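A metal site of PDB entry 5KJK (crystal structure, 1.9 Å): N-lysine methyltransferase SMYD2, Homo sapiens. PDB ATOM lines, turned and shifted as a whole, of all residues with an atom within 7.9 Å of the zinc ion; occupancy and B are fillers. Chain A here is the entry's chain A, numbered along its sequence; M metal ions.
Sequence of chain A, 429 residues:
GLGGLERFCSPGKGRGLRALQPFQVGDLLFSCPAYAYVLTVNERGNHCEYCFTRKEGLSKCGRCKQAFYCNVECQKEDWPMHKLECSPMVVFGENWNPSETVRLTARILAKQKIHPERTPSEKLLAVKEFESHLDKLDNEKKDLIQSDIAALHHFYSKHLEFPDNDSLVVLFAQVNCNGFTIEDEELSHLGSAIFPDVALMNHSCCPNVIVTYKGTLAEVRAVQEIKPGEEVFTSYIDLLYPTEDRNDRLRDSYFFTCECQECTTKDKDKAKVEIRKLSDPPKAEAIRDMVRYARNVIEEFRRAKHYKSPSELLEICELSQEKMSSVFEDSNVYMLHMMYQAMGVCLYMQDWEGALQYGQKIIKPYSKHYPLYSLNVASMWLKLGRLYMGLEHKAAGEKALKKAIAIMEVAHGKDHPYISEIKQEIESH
SG of Cys 64 sits close to N of Gln 66 (3.4 Å). The guanidinium group (NH1) of Arg 63 lies close to the side-chain sulfur (SG) of Cys 86. N of Cys 61 lies within hydrogen-bond range of O of Ala 67 (2.8 Å). The side-chain sulfur (SG) of Cys 61 sits close to the backbone NH (N) of Arg 63 (3.7 Å).
The side-chain sulfur (SG) of Cys 64 is bound to the zinc ion, 2.2 Å away. The zinc ion is bound by NE2 of His 82, at 2.2 Å. The side-chain sulfur (SG) of Cys 86 is bound to the zinc ion, 2.4 Å away. The side-chain sulfur (SG) of Cys 61 is bound to the zinc ion (2.4 Å).
Within 4 Å of the zinc ion: Cys 61, Cys 64, His 82 and Cys 86. The nearest printed residue that does not touch the zinc ion is Ala 67 (4.5 Å).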
ATOM      1  N   LYS A  60      -6.109 -23.439 -17.479  1.00  0.00           N
ATOM      2  CA  LYS A  60      -7.499 -23.901 -17.566  1.00  0.00           C
ATOM      3  C   LYS A  60      -7.603 -25.415 -17.219  1.00  0.00           C
ATOM      4  O   LYS A  60      -6.762 -26.190 -17.689  1.00  0.00           O
ATOM      5  CB  LYS A  60      -7.951 -23.658 -19.009  1.00  0.00           C
ATOM      6  CG  LYS A  60      -9.418 -23.846 -19.331  1.00  0.00           C
ATOM      7  CD  LYS A  60      -9.582 -24.030 -20.833  1.00  0.00           C
ATOM      8  CE  LYS A  60      -9.955 -22.765 -21.572  1.00  0.00           C
ATOM      9  NZ  LYS A  60     -10.176 -23.032 -23.022  1.00  0.00           N
ATOM     10  N   CYS A  61      -8.613 -25.830 -16.405  1.00  0.00           N
ATOM     11  CA  CYS A  61      -8.835 -27.260 -16.113  1.00  0.00           C
ATOM     12  C   CYS A  61      -9.242 -27.876 -17.447  1.00  0.00           C
ATOM     13  O   CYS A  61     -10.138 -27.347 -18.115  1.00  0.00           O
ATOM     14  CB  CYS A  61      -9.921 -27.476 -15.054  1.00  0.00           C
ATOM     15  SG  CYS A  61     -10.460 -29.203 -14.883  1.00  0.00           S
ATOM     16  N   GLY A  62      -8.530 -28.908 -17.852  1.00  0.00           N
ATOM     17  CA  GLY A  62      -8.718 -29.584 -19.131  1.00  0.00           C
ATOM     18  C   GLY A  62     -10.055 -30.264 -19.335  1.00  0.00           C
ATOM     19  O   GLY A  62     -10.488 -30.428 -20.482  1.00  0.00           O
ATOM     20  N   ARG A  63     -10.715 -30.688 -18.248  1.00  0.00           N
ATOM     21  CA  ARG A  63     -11.997 -31.394 -18.361  1.00  0.00           C
ATOM     22  C   ARG A  63     -13.185 -30.461 -18.520  1.00  0.00           C
ATOM     23  O   ARG A  63     -13.954 -30.617 -19.483  1.00  0.00           O
ATOM     24  CB  ARG A  63     -12.197 -32.347 -17.187  1.00  0.00           C
ATOM     25  CG  ARG A  63     -13.515 -33.145 -17.202  1.00  0.00           C
ATOM     26  CD  ARG A  63     -13.618 -34.113 -16.029  1.00  0.00           C
ATOM     27  NE  ARG A  63     -12.428 -34.963 -15.889  1.00  0.00           N
ATOM     28  CZ  ARG A  63     -11.455 -34.761 -15.001  1.00  0.00           C
ATOM     29  NH1 ARG A  63     -11.505 -33.726 -14.166  1.00  0.00           N
ATOM     30  NH2 ARG A  63     -10.403 -35.579 -14.954  1.00  0.00           N
ATOM     31  N   CYS A  64     -13.400 -29.561 -17.540  1.00  0.00           N
ATOM     32  CA  CYS A  64     -14.554 -28.669 -17.574  1.00  0.00           C
ATOM     33  C   CYS A  64     -14.268 -27.407 -18.383  1.00  0.00           C
ATOM     34  O   CYS A  64     -15.213 -26.784 -18.866  1.00  0.00           O
ATOM     35  CB  CYS A  64     -15.014 -28.347 -16.160  1.00  0.00           C
ATOM     36  SG  CYS A  64     -13.783 -27.428 -15.194  1.00  0.00           S
ATOM     37  N   LYS A  65     -12.988 -26.985 -18.458  1.00  0.00           N
ATOM     38  CA  LYS A  65     -12.553 -25.737 -19.115  1.00  0.00           C
ATOM     39  C   LYS A  65     -13.152 -24.478 -18.435  1.00  0.00           C
ATOM     40  O   LYS A  65     -13.157 -23.386 -18.999  1.00  0.00           O
ATOM     41  CB  LYS A  65     -12.809 -25.783 -20.646  1.00  0.00           C
ATOM     42  CG  LYS A  65     -12.022 -26.889 -21.345  1.00  0.00           C
ATOM     43  CD  LYS A  65     -12.663 -27.302 -22.645  1.00  0.00           C
ATOM     44  CE  LYS A  65     -12.078 -28.591 -23.170  1.00  0.00           C
ATOM     45  NZ  LYS A  65     -12.635 -29.781 -22.454  1.00  0.00           N
ATOM     46  N   GLN A  66     -13.656 -24.651 -17.193  1.00  0.00           N
ATOM     47  CA  GLN A  66     -14.340 -23.601 -16.446  1.00  0.00           C
ATOM     48  C   GLN A  66     -13.792 -23.402 -15.027  1.00  0.00           C
ATOM     49  O   GLN A  66     -14.505 -22.953 -14.119  1.00  0.00           O
ATOM     50  CB  GLN A  66     -15.868 -23.835 -16.459  1.00  0.00           C
ATOM     51  CG  GLN A  66     -16.508 -23.615 -17.832  1.00  0.00           C
ATOM     52  CD  GLN A  66     -17.992 -23.884 -17.813  1.00  0.00           C
ATOM     53  OE1 GLN A  66     -18.804 -22.993 -17.553  1.00  0.00           O
ATOM     54  NE2 GLN A  66     -18.388 -25.098 -18.115  1.00  0.00           N
ATOM     55  N   ALA A  67     -12.512 -23.744 -14.837  1.00  0.00           N
ATOM     56  CA  ALA A  67     -11.730 -23.518 -13.611  1.00  0.00           C
ATOM     57  C   ALA A  67     -10.331 -23.180 -14.070  1.00  0.00           C
ATOM     58  O   ALA A  67      -9.830 -23.782 -15.026  1.00  0.00           O
ATOM     59  CB  ALA A  67     -11.713 -24.747 -12.713  1.00  0.00           C
ATOM     60  N   PHE A  68      -9.733 -22.152 -13.457  1.00  0.00           N
ATOM     61  CA  PHE A  68      -8.392 -21.665 -13.830  1.00  0.00           C
ATOM     62  C   PHE A  68      -7.521 -21.597 -12.604  1.00  0.00           C
ATOM     63  O   PHE A  68      -7.997 -21.231 -11.524  1.00  0.00           O
ATOM     64  CB  PHE A  68      -8.467 -20.312 -14.560  1.00  0.00           C
ATOM     65  CG  PHE A  68      -9.284 -20.339 -15.837  1.00  0.00           C
ATOM     66  CD1 PHE A  68      -8.650 -20.317 -17.078  1.00  0.00           C
ATOM     67  CD2 PHE A  68     -10.674 -20.350 -15.804  1.00  0.00           C
ATOM     68  CE1 PHE A  68      -9.408 -20.319 -18.255  1.00  0.00           C
ATOM     69  CE2 PHE A  68     -11.421 -20.360 -16.983  1.00  0.00           C
ATOM     70  CZ  PHE A  68     -10.784 -20.328 -18.205  1.00  0.00           C
ATOM     71  N   TYR A  69      -6.242 -21.972 -12.783  1.00  0.00           N
ATOM     72  CA  TYR A  69      -5.260 -22.071 -11.707  1.00  0.00           C
ATOM     73  C   TYR A  69      -3.928 -21.438 -12.005  1.00  0.00           C
ATOM     74  O   TYR A  69      -3.585 -21.273 -13.181  1.00  0.00           O
ATOM     75  CB  TYR A  69      -5.020 -23.560 -11.383  1.00  0.00           C
ATOM     76  CG  TYR A  69      -6.292 -24.271 -10.967  1.00  0.00           C
ATOM     77  CD1 TYR A  69      -7.003 -25.059 -11.870  1.00  0.00           C
ATOM     78  CD2 TYR A  69      -6.815 -24.104  -9.685  1.00  0.00           C
ATOM     79  CE1 TYR A  69      -8.182 -25.693 -11.493  1.00  0.00           C
ATOM     80  CE2 TYR A  69      -7.968 -24.755  -9.294  1.00  0.00           C
ATOM     81  CZ  TYR A  69      -8.659 -25.540 -10.201  1.00  0.00           C
ATOM     82  OH  TYR A  69      -9.814 -26.170  -9.798  1.00  0.00           O
ATOM     83  N   GLN A  75      -4.153 -26.324  -8.892  1.00  0.00           N
ATOM     84  CA  GLN A  75      -5.126 -27.251  -9.484  1.00  0.00           C
ATOM     85  C   GLN A  75      -5.383 -28.472  -8.599  1.00  0.00           C
ATOM     86  O   GLN A  75      -6.543 -28.764  -8.292  1.00  0.00           O
ATOM     87  CB  GLN A  75      -4.692 -27.678 -10.904  1.00  0.00           C
ATOM     88  CG  GLN A  75      -5.757 -28.523 -11.619  1.00  0.00           C
ATOM     89  CD  GLN A  75      -5.537 -28.748 -13.102  1.00  0.00           C
ATOM     90  OE1 GLN A  75      -6.356 -29.362 -13.794  1.00  0.00           O
ATOM     91  NE2 GLN A  75      -4.403 -28.318 -13.616  1.00  0.00           N
ATOM     92  N   ASP A  78      -6.968 -27.721  -5.167  1.00  0.00           N
ATOM     93  CA  ASP A  78      -8.387 -27.343  -5.295  1.00  0.00           C
ATOM     94  C   ASP A  78      -9.320 -28.519  -5.655  1.00  0.00           C
ATOM     95  O   ASP A  78     -10.537 -28.398  -5.483  1.00  0.00           O
ATOM     96  CB  ASP A  78      -8.540 -26.240  -6.350  1.00  0.00           C
ATOM     97  CG  ASP A  78      -9.904 -25.570  -6.281  1.00  0.00           C
ATOM     98  OD1 ASP A  78     -10.610 -25.529  -7.325  1.00  0.00           O
ATOM     99  OD2 ASP A  78     -10.309 -25.163  -5.175  1.00  0.00           O
ATOM    100  N   TRP A  79      -8.760 -29.609  -6.191  1.00  0.00           N
ATOM    101  CA  TRP A  79      -9.518 -30.782  -6.650  1.00  0.00           C
ATOM    102  C   TRP A  79     -10.531 -31.341  -5.622  1.00  0.00           C
ATOM    103  O   TRP A  79     -11.675 -31.543  -6.044  1.00  0.00           O
ATOM    104  CB  TRP A  79      -8.605 -31.909  -7.161  1.00  0.00           C
ATOM    105  CG  TRP A  79      -9.374 -33.091  -7.678  1.00  0.00           C
ATOM    106  CD1 TRP A  79      -9.416 -34.342  -7.126  1.00  0.00           C
ATOM    107  CD2 TRP A  79     -10.291 -33.101  -8.781  1.00  0.00           C
ATOM    108  NE1 TRP A  79     -10.234 -35.155  -7.873  1.00  0.00           N
ATOM    109  CE2 TRP A  79     -10.793 -34.423  -8.887  1.00  0.00           C
ATOM    110  CE3 TRP A  79     -10.742 -32.125  -9.681  1.00  0.00           C
ATOM    111  CZ2 TRP A  79     -11.698 -34.792  -9.885  1.00  0.00           C
ATOM    112  CZ3 TRP A  79     -11.655 -32.485 -10.656  1.00  0.00           C
ATOM    113  CH2 TRP A  79     -12.143 -33.806 -10.746  1.00  0.00           C
ATOM    114  N   HIS A  82     -13.154 -28.710  -6.193  1.00  0.00           N
ATOM    115  CA  HIS A  82     -13.483 -28.611  -7.614  1.00  0.00           C
ATOM    116  C   HIS A  82     -14.205 -29.843  -8.194  1.00  0.00           C
ATOM    117  O   HIS A  82     -15.055 -29.700  -9.103  1.00  0.00           O
ATOM    118  CB  HIS A  82     -12.239 -28.258  -8.449  1.00  0.00           C
ATOM    119  CG  HIS A  82     -12.569 -28.057  -9.889  1.00  0.00           C
ATOM    120  ND1 HIS A  82     -13.595 -27.217 -10.290  1.00  0.00           N
ATOM    121  CD2 HIS A  82     -12.046 -28.658 -10.983  1.00  0.00           C
ATOM    122  CE1 HIS A  82     -13.662 -27.314 -11.607  1.00  0.00           C
ATOM    123  NE2 HIS A  82     -12.730 -28.135 -12.076  1.00  0.00           N
ATOM    124  N   LYS A  83     -13.933 -31.044  -7.637  1.00  0.00           N
ATOM    125  CA  LYS A  83     -14.577 -32.248  -8.121  1.00  0.00           C
ATOM    126  C   LYS A  83     -16.113 -32.230  -7.923  1.00  0.00           C
ATOM    127  O   LYS A  83     -16.821 -32.904  -8.671  1.00  0.00           O
ATOM    128  CB  LYS A  83     -13.936 -33.533  -7.552  1.00  0.00           C
ATOM    129  CG  LYS A  83     -14.262 -33.920  -6.128  1.00  0.00           C
ATOM    130  CD  LYS A  83     -14.014 -35.407  -6.010  1.00  0.00           C
ATOM    131  CE  LYS A  83     -13.934 -35.871  -4.592  1.00  0.00           C
ATOM    132  NZ  LYS A  83     -13.620 -37.324  -4.528  1.00  0.00           N
ATOM    133  N   GLU A  85     -17.988 -29.921  -8.793  1.00  0.00           N
ATOM    134  CA  GLU A  85     -18.500 -29.186  -9.929  1.00  0.00           C
ATOM    135  C   GLU A  85     -17.929 -29.544 -11.285  1.00  0.00           C
ATOM    136  O   GLU A  85     -18.551 -29.218 -12.292  1.00  0.00           O
ATOM    137  CB  GLU A  85     -18.255 -27.689  -9.672  1.00  0.00           C
ATOM    138  CG  GLU A  85     -19.052 -27.197  -8.490  1.00  0.00           C
ATOM    139  CD  GLU A  85     -18.876 -25.736  -8.147  1.00  0.00           C
ATOM    140  OE1 GLU A  85     -17.901 -25.120  -8.624  1.00  0.00           O
ATOM    141  OE2 GLU A  85     -19.741 -25.211  -7.411  1.00  0.00           O
ATOM    142  N   CYS A  86     -16.716 -30.149 -11.331  1.00  0.00           N
ATOM    143  CA  CYS A  86     -16.028 -30.402 -12.588  1.00  0.00           C
ATOM    144  C   CYS A  86     -16.862 -31.183 -13.627  1.00  0.00           C
ATOM    145  O   CYS A  86     -17.269 -30.589 -14.625  1.00  0.00           O
ATOM    146  CB  CYS A  86     -14.658 -31.055 -12.371  1.00  0.00           C
ATOM    147  SG  CYS A  86     -13.650 -31.113 -13.868  1.00  0.00           S
ATOM    148  N   SER A  87     -17.092 -32.487 -13.414  1.00  0.00           N
ATOM    149  CA  SER A  87     -17.916 -33.262 -14.354  1.00  0.00           C
ATOM    150  C   SER A  87     -19.387 -32.714 -14.397  1.00  0.00           C
ATOM    151  O   SER A  87     -19.904 -32.589 -15.511  1.00  0.00           O
ATOM    152  CB  SER A  87     -17.863 -34.760 -14.040  1.00  0.00           C
ATOM    153  OG  SER A  87     -18.571 -35.461 -15.055  1.00  0.00           O
ATOM    154  N   MET A  89     -20.572 -29.659 -14.401  1.00  0.00           N
ATOM    155  CA  MET A  89     -20.564 -28.554 -15.378  1.00  0.00           C
ATOM    156  C   MET A  89     -20.547 -29.026 -16.842  1.00  0.00           C
ATOM    157  O   MET A  89     -21.210 -28.431 -17.682  1.00  0.00           O
ATOM    158  CB  MET A  89     -19.389 -27.608 -15.135  1.00  0.00           C
ATOM    159  CG  MET A  89     -19.621 -26.638 -13.986  1.00  0.00           C
ATOM    160  SD  MET A  89     -18.372 -25.345 -13.948  1.00  0.00           S
ATOM    161  CE  MET A  89     -16.983 -26.206 -13.176  1.00  0.00           C
ATOM    162  N   VAL A  90     -19.782 -30.084 -17.166  1.00  0.00           N
ATOM    163  CA  VAL A  90     -19.769 -30.508 -18.567  1.00  0.00           C
ATOM    164  C   VAL A  90     -21.060 -31.329 -18.864  1.00  0.00           C
ATOM    165  O   VAL A  90     -21.610 -31.189 -19.971  1.00  0.00           O
ATOM    166  CB  VAL A  90     -18.444 -31.162 -19.098  1.00  0.00           C
ATOM    167  CG1 VAL A  90     -17.373 -31.359 -18.022  1.00  0.00           C
ATOM    168  CG2 VAL A  90     -18.647 -32.398 -19.973  1.00  0.00           C
HETATM  169 ZN    ZN M   1     -12.717 -28.955 -14.086  1.00  0.00          ZN
